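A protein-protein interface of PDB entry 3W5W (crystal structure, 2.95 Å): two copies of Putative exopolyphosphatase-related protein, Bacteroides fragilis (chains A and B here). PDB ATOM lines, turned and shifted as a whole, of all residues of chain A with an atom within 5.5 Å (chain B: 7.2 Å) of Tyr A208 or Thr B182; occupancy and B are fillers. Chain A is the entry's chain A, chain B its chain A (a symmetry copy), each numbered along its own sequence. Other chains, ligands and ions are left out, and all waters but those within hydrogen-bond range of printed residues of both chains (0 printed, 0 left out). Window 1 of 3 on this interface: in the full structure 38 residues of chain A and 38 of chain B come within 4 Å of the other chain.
Printed residues of chain B that touch a printed residue of chain A: Phe B181, Thr B182, Tyr B183, Asn B184, Ser B185 and Tyr B191.
Hydrophobic or aromatic side chains of chain B that line the printed part of chain A: Tyr B191.
Along chain B the printed residues that touch a printed residue of chain A span positions 181 to 191.
Hydrophobic or aromatic side chains of chain A within 4 Å of the printed part of chain B: Tyr A208.
Among the printed residues, no Asp or Glu carboxylate lies within 4 Å of a Lys or Arg side-chain nitrogen of the other chain.
OD1 of Asp A205 is in hydrogen-bond range of N of Tyr B183 (3.3 Å).
The side-chain carboxylate of Asp A205 lies within hydrogen-bond range of the side-chain hydroxyl of Ser B185, at 2.7 Å.
The backbone carbonyl oxygen (O) of Phe B181 sits at hydrogen-bond distance from the side-chain amino group (NZ) of Lys A204, 2.9 Å away.
The guanidinium group (NH1) of Arg A209 sits at hydrogen-bond distance from the backbone carbonyl oxygen (O) of Thr B182 (3.4 Å).
The side-chain carboxylate (OD1) of Asp A205 sits close to the backbone carbonyl oxygen (O) of Thr B182, at 3.2 Å.
NZ of Lys A204 lies within hydrogen-bond range of OG of Ser B185 (2.7 Å).
N of Asn B184 is in hydrogen-bond range of OD2 of Asp A205, at 3.0 Å.
The side-chain amino group (NZ) of Lys A204 is in hydrogen-bond range of the side-chain hydroxyl (OH) of Tyr B191.
3 positions are printed for both chains.
Of the 9 pairs that touch across the chains among the printed residues, none has its exchanged pair printed and touching as well.
Of chain B, only Thr B182 comes within 4 Å of Tyr A208.
Printed residues of chain A within 4 Å of Phe B181: Lys A204.
Printed residues of chain B within 4 Å of Lys A204: Phe B181, Ser B185 and Tyr B191.
Among the printed residues, pairs that only touch across the chains: Tyr A208 with Thr B182 (3.4 Å).
The side-chain amino group (NZ) of Lys A204 lies within salt-bridge range of the side-chain carboxylate (OD1) of Asp A205, 3.9 Å away.
The backbone NH (N) of Tyr B183 is in hydrogen-bond range of the backbone carbonyl oxygen (O) of Thr B178 (3.3 Å).
OG1 of Thr B178 sits at hydrogen-bond distance from N of Phe B181 (2.7 Å).
O of Gly B179 lies within hydrogen-bond range of OG1 of Thr B182.
The backbone carbonyl oxygen (O) of Thr B178 sits at hydrogen-bond distance from the side-chain hydroxyl (OG1) of Thr B182 (3.3 Å).
OH of Tyr B183 sits at hydrogen-bond distance from N of Gly B179 (3.5 Å).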
ATOM      1  N   MET A 175     -13.550  -2.561  24.085  1.00  0.00           N
ATOM      2  CA  MET A 175     -12.775  -3.242  23.059  1.00  0.00           C
ATOM      3  C   MET A 175     -11.287  -3.085  23.352  1.00  0.00           C
ATOM      4  O   MET A 175     -10.545  -4.063  23.397  1.00  0.00           O
ATOM      5  CB  MET A 175     -13.113  -2.665  21.687  1.00  0.00           C
ATOM      6  CG  MET A 175     -12.195  -3.120  20.580  1.00  0.00           C
ATOM      7  SD  MET A 175     -12.579  -2.326  19.017  1.00  0.00           S
ATOM      8  CE  MET A 175     -12.161  -0.602  19.388  1.00  0.00           C
ATOM      9  N   GLY A 180      -9.556  -6.119  21.590  1.00  0.00           N
ATOM     10  CA  GLY A 180     -10.544  -6.696  20.716  1.00  0.00           C
ATOM     11  C   GLY A 180     -11.184  -7.923  21.337  1.00  0.00           C
ATOM     12  O   GLY A 180     -11.547  -8.870  20.637  1.00  0.00           O
ATOM     13  N   ASP A 203     -21.607   0.705  14.897  1.00  0.00           N
ATOM     14  CA  ASP A 203     -21.062  -0.228  13.928  1.00  0.00           C
ATOM     15  C   ASP A 203     -19.760  -0.689  14.565  1.00  0.00           C
ATOM     16  O   ASP A 203     -18.733  -0.037  14.409  1.00  0.00           O
ATOM     17  CB  ASP A 203     -20.763   0.490  12.612  1.00  0.00           C
ATOM     18  CG  ASP A 203     -20.180  -0.436  11.554  1.00  0.00           C
ATOM     19  OD1 ASP A 203     -19.411  -1.353  11.908  1.00  0.00           O
ATOM     20  OD2 ASP A 203     -20.471  -0.241  10.359  1.00  0.00           O
ATOM     21  N   LYS A 204     -19.793  -1.801  15.290  1.00  0.00           N
ATOM     22  CA  LYS A 204     -18.584  -2.266  15.946  1.00  0.00           C
ATOM     23  C   LYS A 204     -17.462  -2.508  14.964  1.00  0.00           C
ATOM     24  O   LYS A 204     -16.313  -2.183  15.244  1.00  0.00           O
ATOM     25  CB  LYS A 204     -18.849  -3.528  16.772  1.00  0.00           C
ATOM     26  CG  LYS A 204     -19.453  -4.681  16.020  1.00  0.00           C
ATOM     27  CD  LYS A 204     -19.776  -5.816  16.987  1.00  0.00           C
ATOM     28  CE  LYS A 204     -18.513  -6.418  17.584  1.00  0.00           C
ATOM     29  NZ  LYS A 204     -17.688  -7.097  16.533  1.00  0.00           N
ATOM     30  N   ASP A 205     -17.782  -3.055  13.801  1.00  0.00           N
ATOM     31  CA  ASP A 205     -16.733  -3.310  12.831  1.00  0.00           C
ATOM     32  C   ASP A 205     -15.996  -2.035  12.421  1.00  0.00           C
ATOM     33  O   ASP A 205     -14.774  -2.045  12.251  1.00  0.00           O
ATOM     34  CB  ASP A 205     -17.308  -4.023  11.615  1.00  0.00           C
ATOM     35  CG  ASP A 205     -17.789  -5.410  11.948  1.00  0.00           C
ATOM     36  OD1 ASP A 205     -17.180  -6.030  12.838  1.00  0.00           O
ATOM     37  OD2 ASP A 205     -18.761  -5.894  11.327  1.00  0.00           O
ATOM     38  N   ASP A 206     -16.728  -0.936  12.289  1.00  0.00           N
ATOM     39  CA  ASP A 206     -16.124   0.336  11.904  1.00  0.00           C
ATOM     40  C   ASP A 206     -15.249   0.904  13.022  1.00  0.00           C
ATOM     41  O   ASP A 206     -14.130   1.348  12.763  1.00  0.00           O
ATOM     42  CB  ASP A 206     -17.209   1.351  11.520  1.00  0.00           C
ATOM     43  CG  ASP A 206     -16.627   2.661  11.008  1.00  0.00           C
ATOM     44  OD1 ASP A 206     -15.799   2.621  10.068  1.00  0.00           O
ATOM     45  OD2 ASP A 206     -16.998   3.730  11.543  1.00  0.00           O
ATOM     46  N   ILE A 207     -15.766   0.888  14.252  1.00  0.00           N
ATOM     47  CA  ILE A 207     -15.043   1.370  15.429  1.00  0.00           C
ATOM     48  C   ILE A 207     -13.723   0.633  15.488  1.00  0.00           C
ATOM     49  O   ILE A 207     -12.681   1.211  15.809  1.00  0.00           O
ATOM     50  CB  ILE A 207     -15.846   1.098  16.740  1.00  0.00           C
ATOM     51  CG1 ILE A 207     -16.987   2.108  16.856  1.00  0.00           C
ATOM     52  CG2 ILE A 207     -14.945   1.179  17.965  1.00  0.00           C
ATOM     53  CD1 ILE A 207     -17.794   1.995  18.110  1.00  0.00           C
ATOM     54  N   TYR A 208     -13.772  -0.650  15.160  1.00  0.00           N
ATOM     55  CA  TYR A 208     -12.572  -1.466  15.155  1.00  0.00           C
ATOM     56  C   TYR A 208     -11.560  -0.888  14.167  1.00  0.00           C
ATOM     57  O   TYR A 208     -10.439  -0.560  14.541  1.00  0.00           O
ATOM     58  CB  TYR A 208     -12.893  -2.907  14.759  1.00  0.00           C
ATOM     59  CG  TYR A 208     -11.682  -3.813  14.822  1.00  0.00           C
ATOM     60  CD1 TYR A 208     -11.181  -4.259  16.051  1.00  0.00           C
ATOM     61  CD2 TYR A 208     -10.983  -4.146  13.662  1.00  0.00           C
ATOM     62  CE1 TYR A 208     -10.012  -5.006  16.121  1.00  0.00           C
ATOM     63  CE2 TYR A 208      -9.813  -4.886  13.718  1.00  0.00           C
ATOM     64  CZ  TYR A 208      -9.329  -5.310  14.948  1.00  0.00           C
ATOM     65  OH  TYR A 208      -8.145  -6.012  14.998  1.00  0.00           O
ATOM     66  N   ARG A 209     -11.954  -0.759  12.907  1.00  0.00           N
ATOM     67  CA  ARG A 209     -11.049  -0.228  11.900  1.00  0.00           C
ATOM     68  C   ARG A 209     -10.520   1.166  12.207  1.00  0.00           C
ATOM     69  O   ARG A 209      -9.372   1.483  11.891  1.00  0.00           O
ATOM     70  CB  ARG A 209     -11.719  -0.231  10.519  1.00  0.00           C
ATOM     71  CG  ARG A 209     -11.648  -1.584   9.820  1.00  0.00           C
ATOM     72  CD  ARG A 209     -12.280  -1.541   8.438  1.00  0.00           C
ATOM     73  NE  ARG A 209     -13.746  -1.544   8.474  1.00  0.00           N
ATOM     74  CZ  ARG A 209     -14.505  -2.606   8.757  1.00  0.00           C
ATOM     75  NH1 ARG A 209     -13.954  -3.784   9.041  1.00  0.00           N
ATOM     76  NH2 ARG A 209     -15.826  -2.493   8.741  1.00  0.00           N
ATOM     77  N   LYS A 210     -11.340   2.001  12.830  1.00  0.00           N
ATOM     78  CA  LYS A 210     -10.915   3.358  13.133  1.00  0.00           C
ATOM     79  C   LYS A 210      -9.818   3.443  14.186  1.00  0.00           C
ATOM     80  O   LYS A 210      -9.116   4.449  14.286  1.00  0.00           O
ATOM     81  CB  LYS A 210     -12.132   4.188  13.537  1.00  0.00           C
ATOM     82  CG  LYS A 210     -13.038   4.457  12.350  1.00  0.00           C
ATOM     83  CD  LYS A 210     -14.468   4.730  12.739  1.00  0.00           C
ATOM     84  CE  LYS A 210     -14.618   6.085  13.357  1.00  0.00           C
ATOM     85  NZ  LYS A 210     -16.055   6.362  13.600  1.00  0.00           N
ATOM     86  N   VAL A 211      -9.650   2.371  14.947  1.00  0.00           N
ATOM     87  CA  VAL A 211      -8.647   2.328  16.005  1.00  0.00           C
ATOM     88  C   VAL A 211      -7.408   1.487  15.655  1.00  0.00           C
ATOM     89  O   VAL A 211      -6.269   1.881  15.915  1.00  0.00           O
ATOM     90  CB  VAL A 211      -9.280   1.759  17.314  1.00  0.00           C
ATOM     91  CG1 VAL A 211      -8.241   1.632  18.411  1.00  0.00           C
ATOM     92  CG2 VAL A 211     -10.418   2.647  17.759  1.00  0.00           C
ATOM     93  N   TYR A 212      -7.640   0.338  15.041  1.00  0.00           N
ATOM     94  CA  TYR A 212      -6.565  -0.578  14.729  1.00  0.00           C
ATOM     95  C   TYR A 212      -6.113  -0.664  13.278  1.00  0.00           C
ATOM     96  O   TYR A 212      -4.981  -1.063  13.010  1.00  0.00           O
ATOM     97  CB  TYR A 212      -6.970  -1.968  15.193  1.00  0.00           C
ATOM     98  CG  TYR A 212      -7.239  -2.092  16.673  1.00  0.00           C
ATOM     99  CD1 TYR A 212      -6.193  -2.142  17.584  1.00  0.00           C
ATOM    100  CD2 TYR A 212      -8.542  -2.238  17.161  1.00  0.00           C
ATOM    101  CE1 TYR A 212      -6.431  -2.349  18.944  1.00  0.00           C
ATOM    102  CE2 TYR A 212      -8.789  -2.447  18.522  1.00  0.00           C
ATOM    103  CZ  TYR A 212      -7.726  -2.508  19.404  1.00  0.00           C
ATOM    104  OH  TYR A 212      -7.936  -2.771  20.740  1.00  0.00           O
ATOM    105  N   ASN A 213      -6.982  -0.307  12.340  1.00  0.00           N
ATOM    106  CA  ASN A 213      -6.622  -0.408  10.934  1.00  0.00           C
ATOM    107  C   ASN A 213      -6.544   0.930  10.247  1.00  0.00           C
ATOM    108  O   ASN A 213      -7.133   1.138   9.186  1.00  0.00           O
ATOM    109  CB  ASN A 213      -7.617  -1.305  10.218  1.00  0.00           C
ATOM    110  CG  ASN A 213      -7.627  -2.707  10.776  1.00  0.00           C
ATOM    111  OD1 ASN A 213      -8.619  -3.422  10.655  1.00  0.00           O
ATOM    112  ND2 ASN A 213      -6.517  -3.113  11.389  1.00  0.00           N
ATOM    113  N   MET B 175     -15.612 -17.381  15.075  1.00  0.00           N
ATOM    114  CA  MET B 175     -14.504 -16.460  15.275  1.00  0.00           C
ATOM    115  C   MET B 175     -13.710 -16.326  13.982  1.00  0.00           C
ATOM    116  O   MET B 175     -13.464 -15.222  13.502  1.00  0.00           O
ATOM    117  CB  MET B 175     -13.607 -16.966  16.402  1.00  0.00           C
ATOM    118  CG  MET B 175     -12.298 -16.227  16.532  1.00  0.00           C
ATOM    119  SD  MET B 175     -11.248 -16.936  17.802  1.00  0.00           S
ATOM    120  CE  MET B 175     -10.879 -18.560  17.086  1.00  0.00           C
ATOM    121  N   ASP B 177     -14.423 -16.974  10.718  1.00  0.00           N
ATOM    122  CA  ASP B 177     -15.051 -16.301   9.591  1.00  0.00           C
ATOM    123  C   ASP B 177     -15.330 -14.822   9.773  1.00  0.00           C
ATOM    124  O   ASP B 177     -15.831 -14.166   8.864  1.00  0.00           O
ATOM    125  CB  ASP B 177     -16.333 -17.032   9.202  1.00  0.00           C
ATOM    126  CG  ASP B 177     -16.134 -17.951   8.016  1.00  0.00           C
ATOM    127  OD1 ASP B 177     -14.980 -18.392   7.782  1.00  0.00           O
ATOM    128  OD2 ASP B 177     -17.135 -18.240   7.327  1.00  0.00           O
ATOM    129  N   THR B 178     -14.997 -14.291  10.938  1.00  0.00           N
ATOM    130  CA  THR B 178     -15.217 -12.878  11.212  1.00  0.00           C
ATOM    131  C   THR B 178     -13.898 -12.235  11.603  1.00  0.00           C
ATOM    132  O   THR B 178     -13.864 -11.068  12.000  1.00  0.00           O
ATOM    133  CB  THR B 178     -16.219 -12.676  12.374  1.00  0.00           C
ATOM    134  OG1 THR B 178     -15.735 -13.328  13.565  1.00  0.00           O
ATOM    135  CG2 THR B 178     -17.583 -13.225  11.988  1.00  0.00           C
ATOM    136  N   GLY B 179     -12.815 -13.002  11.482  1.00  0.00           N
ATOM    137  CA  GLY B 179     -11.510 -12.496  11.860  1.00  0.00           C
ATOM    138  C   GLY B 179     -11.606 -11.963  13.275  1.00  0.00           C
ATOM    139  O   GLY B 179     -11.400 -10.776  13.530  1.00  0.00           O
ATOM    140  N   GLY B 180     -11.939 -12.845  14.205  1.00  0.00           N
ATOM    141  CA  GLY B 180     -12.072 -12.411  15.572  1.00  0.00           C
ATOM    142  C   GLY B 180     -13.200 -11.410  15.727  1.00  0.00           C
ATOM    143  O   GLY B 180     -13.130 -10.500  16.556  1.00  0.00           O
ATOM    144  N   PHE B 181     -14.257 -11.572  14.938  1.00  0.00           N
ATOM    145  CA  PHE B 181     -15.394 -10.663  15.028  1.00  0.00           C
ATOM    146  C   PHE B 181     -14.970  -9.206  14.807  1.00  0.00           C
ATOM    147  O   PHE B 181     -15.272  -8.329  15.617  1.00  0.00           O
ATOM    148  CB  PHE B 181     -16.071 -10.811  16.398  1.00  0.00           C
ATOM    149  CG  PHE B 181     -16.533 -12.207  16.692  1.00  0.00           C
ATOM    150  CD1 PHE B 181     -17.691 -12.702  16.126  1.00  0.00           C
ATOM    151  CD2 PHE B 181     -15.783 -13.041  17.498  1.00  0.00           C
ATOM    152  CE1 PHE B 181     -18.099 -14.016  16.354  1.00  0.00           C
ATOM    153  CE2 PHE B 181     -16.177 -14.346  17.733  1.00  0.00           C
ATOM    154  CZ  PHE B 181     -17.342 -14.836  17.159  1.00  0.00           C
ATOM    155  N   THR B 182     -14.259  -8.965  13.708  1.00  0.00           N
ATOM    156  CA  THR B 182     -13.804  -7.624  13.338  1.00  0.00           C
ATOM    157  C   THR B 182     -14.421  -7.220  12.000  1.00  0.00           C
ATOM    158  O   THR B 182     -14.220  -6.106  11.522  1.00  0.00           O
ATOM    159  CB  THR B 182     -12.269  -7.537  13.215  1.00  0.00           C
ATOM    160  OG1 THR B 182     -11.802  -8.495  12.250  1.00  0.00           O
ATOM    161  CG2 THR B 182     -11.621  -7.783  14.567  1.00  0.00           C
ATOM    162  N   TYR B 183     -15.146  -8.144  11.384  1.00  0.00           N
ATOM    163  CA  TYR B 183     -15.830  -7.846  10.143  1.00  0.00           C
ATOM    164  C   TYR B 183     -17.031  -8.755   9.927  1.00  0.00           C
ATOM    165  O   TYR B 183     -16.983  -9.959  10.186  1.00  0.00           O
ATOM    166  CB  TYR B 183     -14.881  -7.881   8.932  1.00  0.00           C
ATOM    167  CG  TYR B 183     -14.062  -9.136   8.749  1.00  0.00           C
ATOM    168  CD1 TYR B 183     -12.819  -9.283   9.379  1.00  0.00           C
ATOM    169  CD2 TYR B 183     -14.515 -10.178   7.924  1.00  0.00           C
ATOM    170  CE1 TYR B 183     -12.041 -10.437   9.194  1.00  0.00           C
ATOM    171  CE2 TYR B 183     -13.746 -11.342   7.733  1.00  0.00           C
ATOM    172  CZ  TYR B 183     -12.510 -11.466   8.374  1.00  0.00           C
ATOM    173  OH  TYR B 183     -11.755 -12.613   8.210  1.00  0.00           O
ATOM    174  N   ASN B 184     -18.118  -8.133   9.478  1.00  0.00           N
ATOM    175  CA  ASN B 184     -19.391  -8.790   9.213  1.00  0.00           C
ATOM    176  C   ASN B 184     -19.891  -9.399  10.514  1.00  0.00           C
ATOM    177  O   ASN B 184     -20.378 -10.532  10.545  1.00  0.00           O
ATOM    178  CB  ASN B 184     -19.219  -9.858   8.116  1.00  0.00           C
ATOM    179  CG  ASN B 184     -20.539 -10.201   7.413  1.00  0.00           C
ATOM    180  OD1 ASN B 184     -21.410  -9.336   7.233  1.00  0.00           O
ATOM    181  ND2 ASN B 184     -20.680 -11.463   7.000  1.00  0.00           N
ATOM    182  N   SER B 185     -19.786  -8.623  11.591  1.00  0.00           N
ATOM    183  CA  SER B 185     -20.195  -9.102  12.904  1.00  0.00           C
ATOM    184  C   SER B 185     -21.103  -8.131  13.644  1.00  0.00           C
ATOM    185  O   SER B 185     -21.290  -8.243  14.859  1.00  0.00           O
ATOM    186  CB  SER B 185     -18.956  -9.365  13.758  1.00  0.00           C
ATOM    187  OG  SER B 185     -18.315  -8.146  14.081  1.00  0.00           O
ATOM    188  N   TYR B 191     -23.667 -12.073  19.355  1.00  0.00           N
ATOM    189  CA  TYR B 191     -23.232 -11.975  20.740  1.00  0.00           C
ATOM    190  C   TYR B 191     -24.116 -12.695  21.759  1.00  0.00           C
ATOM    191  O   TYR B 191     -23.663 -13.009  22.860  1.00  0.00           O
ATOM    192  CB  TYR B 191     -23.021 -10.492  21.058  1.00  0.00           C
ATOM    193  CG  TYR B 191     -22.088  -9.922  20.018  1.00  0.00           C
ATOM    194  CD1 TYR B 191     -20.717 -10.142  20.102  1.00  0.00           C
ATOM    195  CD2 TYR B 191     -22.589  -9.367  18.837  1.00  0.00           C
ATOM    196  CE1 TYR B 191     -19.871  -9.849  19.034  1.00  0.00           C
ATOM    197  CE2 TYR B 191     -21.752  -9.070  17.758  1.00  0.00           C
ATOM    198  CZ  TYR B 191     -20.394  -9.322  17.863  1.00  0.00           C
ATOM    199  OH  TYR B 191     -19.566  -9.103  16.784  1.00  0.00           O
ATOM    200  N   TYR B 208      -8.874 -18.461  21.141  1.00  0.00           N
ATOM    201  CA  TYR B 208      -8.258 -17.414  20.349  1.00  0.00           C
ATOM    202  C   TYR B 208      -6.756 -17.671  20.234  1.00  0.00           C
ATOM    203  O   TYR B 208      -6.224 -17.787  19.136  1.00  0.00           O
ATOM    204  CB  TYR B 208      -8.484 -16.042  20.986  1.00  0.00           C
ATOM    205  CG  TYR B 208      -7.928 -14.911  20.148  1.00  0.00           C
ATOM    206  CD1 TYR B 208      -8.588 -14.484  18.987  1.00  0.00           C
ATOM    207  CD2 TYR B 208      -6.699 -14.331  20.461  1.00  0.00           C
ATOM    208  CE1 TYR B 208      -8.031 -13.518  18.160  1.00  0.00           C
ATOM    209  CE2 TYR B 208      -6.131 -13.370  19.642  1.00  0.00           C
ATOM    210  CZ  TYR B 208      -6.797 -12.969  18.492  1.00  0.00           C
ATOM    211  OH  TYR B 208      -6.206 -12.040  17.663  1.00  0.00           O
